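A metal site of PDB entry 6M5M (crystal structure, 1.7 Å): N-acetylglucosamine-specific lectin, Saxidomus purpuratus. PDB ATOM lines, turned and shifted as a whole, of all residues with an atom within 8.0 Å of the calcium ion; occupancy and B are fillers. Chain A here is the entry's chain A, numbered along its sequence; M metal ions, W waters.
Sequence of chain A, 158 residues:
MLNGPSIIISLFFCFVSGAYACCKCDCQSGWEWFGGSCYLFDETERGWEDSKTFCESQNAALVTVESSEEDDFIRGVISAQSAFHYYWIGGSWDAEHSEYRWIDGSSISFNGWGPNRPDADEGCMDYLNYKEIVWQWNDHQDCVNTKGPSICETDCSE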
ATOM      1  N   PHE A  34      17.675  12.133  21.893  1.00  0.00           N
ATOM      2  CA  PHE A  34      16.824  12.857  20.928  1.00  0.00           C
ATOM      3  C   PHE A  34      16.199  11.859  19.951  1.00  0.00           C
ATOM      4  O   PHE A  34      16.916  10.995  19.389  1.00  0.00           O
ATOM      5  CB  PHE A  34      17.561  13.988  20.204  1.00  0.00           C
ATOM      6  CG  PHE A  34      16.688  14.614  19.138  1.00  0.00           C
ATOM      7  CD1 PHE A  34      15.759  15.597  19.457  1.00  0.00           C
ATOM      8  CD2 PHE A  34      16.703  14.145  17.833  1.00  0.00           C
ATOM      9  CE1 PHE A  34      14.931  16.145  18.488  1.00  0.00           C
ATOM     10  CE2 PHE A  34      15.862  14.685  16.872  1.00  0.00           C
ATOM     11  CZ  PHE A  34      14.976  15.680  17.194  1.00  0.00           C
ATOM     12  N   GLY A  35      14.868  11.977  19.770  1.00  0.00           N
ATOM     13  CA  GLY A  35      14.110  11.215  18.775  1.00  0.00           C
ATOM     14  C   GLY A  35      14.424   9.730  18.789  1.00  0.00           C
ATOM     15  O   GLY A  35      14.628   9.180  17.689  1.00  0.00           O
ATOM     16  N   SER A  37      16.960   8.062  20.108  1.00  0.00           N
ATOM     17  CA  SER A  37      18.429   7.792  20.054  1.00  0.00           C
ATOM     18  C   SER A  37      19.149   8.539  21.166  1.00  0.00           C
ATOM     19  O   SER A  37      18.739   9.660  21.507  1.00  0.00           O
ATOM     20  CB  SER A  37      19.006   8.211  18.737  1.00  0.00           C
ATOM     21  OG  SER A  37      18.621   7.310  17.722  1.00  0.00           O
ATOM     22  N   TYR A  39      22.949  10.166  21.755  1.00  0.00           N
ATOM     23  CA  TYR A  39      24.096  10.704  21.005  1.00  0.00           C
ATOM     24  C   TYR A  39      25.240  11.022  21.956  1.00  0.00           C
ATOM     25  O   TYR A  39      25.015  11.352  23.156  1.00  0.00           O
ATOM     26  CB  TYR A  39      23.669  11.971  20.272  1.00  0.00           C
ATOM     27  CG  TYR A  39      22.509  11.746  19.328  1.00  0.00           C
ATOM     28  CD1 TYR A  39      21.213  11.583  19.799  1.00  0.00           C
ATOM     29  CD2 TYR A  39      22.710  11.781  17.966  1.00  0.00           C
ATOM     30  CE1 TYR A  39      20.156  11.386  18.924  1.00  0.00           C
ATOM     31  CE2 TYR A  39      21.664  11.584  17.082  1.00  0.00           C
ATOM     32  CZ  TYR A  39      20.384  11.398  17.551  1.00  0.00           C
ATOM     33  OH  TYR A  39      19.377  11.185  16.658  1.00  0.00           O
ATOM     34  N   LEU A  62      28.820   5.459  14.392  1.00  0.00           N
ATOM     35  CA  LEU A  62      28.778   6.886  13.998  1.00  0.00           C
ATOM     36  C   LEU A  62      27.343   7.243  13.609  1.00  0.00           C
ATOM     37  O   LEU A  62      26.575   6.336  13.195  1.00  0.00           O
ATOM     38  CB  LEU A  62      29.701   7.166  12.810  1.00  0.00           C
ATOM     39  CG  LEU A  62      31.186   7.101  13.146  1.00  0.00           C
ATOM     40  CD1 LEU A  62      31.967   6.976  11.856  1.00  0.00           C
ATOM     41  CD2 LEU A  62      31.600   8.357  13.901  1.00  0.00           C
ATOM     42  N   VAL A  63      26.999   8.517  13.726  1.00  0.00           N
ATOM     43  CA  VAL A  63      25.577   8.907  13.613  1.00  0.00           C
ATOM     44  C   VAL A  63      25.153   8.808  12.141  1.00  0.00           C
ATOM     45  O   VAL A  63      25.926   9.194  11.276  1.00  0.00           O
ATOM     46  CB  VAL A  63      25.324  10.308  14.179  1.00  0.00           C
ATOM     47  CG1 VAL A  63      26.117  11.341  13.419  1.00  0.00           C
ATOM     48  CG2 VAL A  63      23.845  10.688  14.162  1.00  0.00           C
ATOM     49  N   THR A  64      23.888   8.453  11.904  1.00  0.00           N
ATOM     50  CA  THR A  64      23.177   8.445  10.594  1.00  0.00           C
ATOM     51  C   THR A  64      22.005   9.435  10.707  1.00  0.00           C
ATOM     52  O   THR A  64      21.367   9.504  11.810  1.00  0.00           O
ATOM     53  CB  THR A  64      22.730   6.998  10.303  1.00  0.00           C
ATOM     54  OG1 THR A  64      21.923   6.458  11.355  1.00  0.00           O
ATOM     55  CG2 THR A  64      23.905   6.065  10.125  1.00  0.00           C
ATOM     56  N   VAL A  65      21.791  10.264   9.719  1.00  0.00           N
ATOM     57  CA  VAL A  65      20.832  11.388   9.886  1.00  0.00           C
ATOM     58  C   VAL A  65      19.698  11.184   8.896  1.00  0.00           C
ATOM     59  O   VAL A  65      19.881  11.531   7.710  1.00  0.00           O
ATOM     60  CB  VAL A  65      21.519  12.741   9.690  1.00  0.00           C
ATOM     61  CG1 VAL A  65      20.595  13.892  10.044  1.00  0.00           C
ATOM     62  CG2 VAL A  65      22.817  12.845  10.492  1.00  0.00           C
ATOM     63  N   GLU A  66      18.560  10.689   9.378  1.00  0.00           N
ATOM     64  CA  GLU A  66      17.444  10.249   8.489  1.00  0.00           C
ATOM     65  C   GLU A  66      16.420  11.368   8.281  1.00  0.00           C
ATOM     66  O   GLU A  66      15.565  11.160   7.397  1.00  0.00           O
ATOM     67  CB  GLU A  66      16.767   9.002   9.057  1.00  0.00           C
ATOM     68  CG  GLU A  66      17.605   7.756   8.881  1.00  0.00           C
ATOM     69  CD  GLU A  66      18.682   7.566   9.936  1.00  0.00           C
ATOM     70  OE1 GLU A  66      18.605   8.210  11.011  1.00  0.00           O
ATOM     71  OE2 GLU A  66      19.574   6.755   9.700  1.00  0.00           O
ATOM     72  N   SER A  67      16.488  12.488   9.013  1.00  0.00           N
ATOM     73  CA  SER A  67      15.454  13.540   8.989  1.00  0.00           C
ATOM     74  C   SER A  67      16.034  14.928   9.252  1.00  0.00           C
ATOM     75  O   SER A  67      17.106  15.023   9.888  1.00  0.00           O
ATOM     76  CB  SER A  67      14.387  13.252   9.966  1.00  0.00           C
ATOM     77  OG  SER A  67      14.889  13.343  11.281  1.00  0.00           O
ATOM     78  N   GLU A  70      16.418  15.520  13.116  1.00  0.00           N
ATOM     79  CA  GLU A  70      17.741  15.007  13.615  1.00  0.00           C
ATOM     80  C   GLU A  70      18.847  16.016  13.234  1.00  0.00           C
ATOM     81  O   GLU A  70      19.663  16.354  14.096  1.00  0.00           O
ATOM     82  CB  GLU A  70      18.087  13.621  13.066  1.00  0.00           C
ATOM     83  CG  GLU A  70      19.121  12.868  13.910  1.00  0.00           C
ATOM     84  CD  GLU A  70      19.317  11.380  13.615  1.00  0.00           C
ATOM     85  OE1 GLU A  70      19.931  10.655  14.435  1.00  0.00           O
ATOM     86  OE2 GLU A  70      18.837  10.943  12.583  1.00  0.00           O
ATOM     87  N   ASP A  71      18.866  16.456  11.986  1.00  0.00           N
ATOM     88  CA  ASP A  71      19.888  17.402  11.444  1.00  0.00           C
ATOM     89  C   ASP A  71      19.908  18.647  12.335  1.00  0.00           C
ATOM     90  O   ASP A  71      20.972  19.122  12.721  1.00  0.00           O
ATOM     91  CB  ASP A  71      19.578  17.630   9.977  1.00  0.00           C
ATOM     92  CG  ASP A  71      20.498  18.595   9.300  1.00  0.00           C
ATOM     93  OD1 ASP A  71      21.690  18.276   9.154  1.00  0.00           O
ATOM     94  OD2 ASP A  71      20.006  19.619   8.874  1.00  0.00           O
ATOM     95  N   ILE A  74      21.305  18.067  15.809  1.00  0.00           N
ATOM     96  CA  ILE A  74      22.785  17.972  15.709  1.00  0.00           C
ATOM     97  C   ILE A  74      23.327  19.392  15.591  1.00  0.00           C
ATOM     98  O   ILE A  74      24.272  19.739  16.351  1.00  0.00           O
ATOM     99  CB  ILE A  74      23.202  17.082  14.523  1.00  0.00           C
ATOM    100  CG1 ILE A  74      22.906  15.599  14.782  1.00  0.00           C
ATOM    101  CG2 ILE A  74      24.675  17.322  14.230  1.00  0.00           C
ATOM    102  CD1 ILE A  74      23.056  14.728  13.521  1.00  0.00           C
ATOM    103  N   TRP A 102      24.751   5.744   4.327  1.00  0.00           N
ATOM    104  CA  TRP A 102      24.950   5.575   5.783  1.00  0.00           C
ATOM    105  C   TRP A 102      25.687   4.256   6.018  1.00  0.00           C
ATOM    106  O   TRP A 102      25.599   3.347   5.131  1.00  0.00           O
ATOM    107  CB  TRP A 102      23.603   5.671   6.504  1.00  0.00           C
ATOM    108  CG  TRP A 102      22.971   7.020   6.318  1.00  0.00           C
ATOM    109  CD1 TRP A 102      21.715   7.266   5.831  1.00  0.00           C
ATOM    110  CD2 TRP A 102      23.554   8.305   6.593  1.00  0.00           C
ATOM    111  NE1 TRP A 102      21.504   8.619   5.752  1.00  0.00           N
ATOM    112  CE2 TRP A 102      22.604   9.274   6.225  1.00  0.00           C
ATOM    113  CE3 TRP A 102      24.773   8.720   7.134  1.00  0.00           C
ATOM    114  CZ2 TRP A 102      22.852  10.645   6.366  1.00  0.00           C
ATOM    115  CZ3 TRP A 102      25.019  10.072   7.264  1.00  0.00           C
ATOM    116  CH2 TRP A 102      24.056  11.023   6.904  1.00  0.00           C
ATOM    117  N   ASP A 104      25.340   1.829   7.973  1.00  0.00           N
ATOM    118  CA  ASP A 104      24.458   0.627   8.079  1.00  0.00           C
ATOM    119  C   ASP A 104      24.009   0.149   6.685  1.00  0.00           C
ATOM    120  O   ASP A 104      23.156  -0.738   6.638  1.00  0.00           O
ATOM    121  CB  ASP A 104      23.248   0.919   8.966  1.00  0.00           C
ATOM    122  CG  ASP A 104      22.312   1.985   8.416  1.00  0.00           C
ATOM    123  OD1 ASP A 104      22.556   2.478   7.306  1.00  0.00           O
ATOM    124  OD2 ASP A 104      21.337   2.307   9.129  1.00  0.00           O
ATOM    125  N   GLU A 153      25.863   7.381  17.774  1.00  0.00           N
ATOM    126  CA  GLU A 153      24.390   7.233  17.954  1.00  0.00           C
ATOM    127  C   GLU A 153      24.105   5.787  18.347  1.00  0.00           C
ATOM    128  O   GLU A 153      24.728   4.900  17.747  1.00  0.00           O
ATOM    129  CB  GLU A 153      23.659   7.603  16.664  1.00  0.00           C
ATOM    130  CG  GLU A 153      22.160   7.327  16.731  1.00  0.00           C
ATOM    131  CD  GLU A 153      21.385   7.760  15.505  1.00  0.00           C
ATOM    132  OE1 GLU A 153      21.969   7.730  14.401  1.00  0.00           O
ATOM    133  OE2 GLU A 153      20.168   8.105  15.631  1.00  0.00           O
ATOM    134  N   THR A 154      23.209   5.553  19.319  1.00  0.00           N
ATOM    135  CA  THR A 154      22.603   4.221  19.592  1.00  0.00           C
ATOM    136  C   THR A 154      21.089   4.414  19.677  1.00  0.00           C
ATOM    137  O   THR A 154      20.643   5.470  20.122  1.00  0.00           O
ATOM    138  CB  THR A 154      23.253   3.584  20.824  1.00  0.00           C
ATOM    139  OG1 THR A 154      22.743   2.256  20.993  1.00  0.00           O
ATOM    140  CG2 THR A 154      23.025   4.354  22.102  1.00  0.00           C
ATOM    141  N   ASP A 155      20.333   3.440  19.198  1.00  0.00           N
ATOM    142  CA  ASP A 155      18.861   3.354  19.363  1.00  0.00           C
ATOM    143  C   ASP A 155      18.588   2.301  20.423  1.00  0.00           C
ATOM    144  O   ASP A 155      17.425   1.941  20.604  1.00  0.00           O
ATOM    145  CB  ASP A 155      18.181   3.154  17.998  1.00  0.00           C
ATOM    146  CG  ASP A 155      18.462   1.822  17.309  1.00  0.00           C
ATOM    147  OD1 ASP A 155      18.882   0.866  17.997  1.00  0.00           O
ATOM    148  OD2 ASP A 155      18.223   1.751  16.092  1.00  0.00           O
HETATM  149 CA    CA M   1      19.726   8.625  13.235  1.00  0.00          CA
HETATM  150  O   HOH W   1      17.673   8.874  13.524  1.00  0.00           O
HETATM  151  O   HOH W   2      19.795   5.942  13.425  1.00  0.00           O
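The backbone NH of Glu 70 sits at hydrogen-bond distance from the side-chain hydroxyl of Ser 67, at 3.2 Å.
The side-chain carboxylate (OE2) of Glu 153 sits close to the side-chain hydroxyl (OH) of Tyr 39, at 3.3 Å.
OE2 of Glu 153 lies close to OG of Ser 37 (2.7 Å).
The nearest printed residue that does not touch the calcium ion is Tyr 39 (4.3 Å).
The calcium ion is bound by water W1, O of Thr 64, OE1 of Glu 70, OE2 of Glu 153, OE1 of Glu 66, OE2 of Glu 70, OE1 of Glu 153 and water W2.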
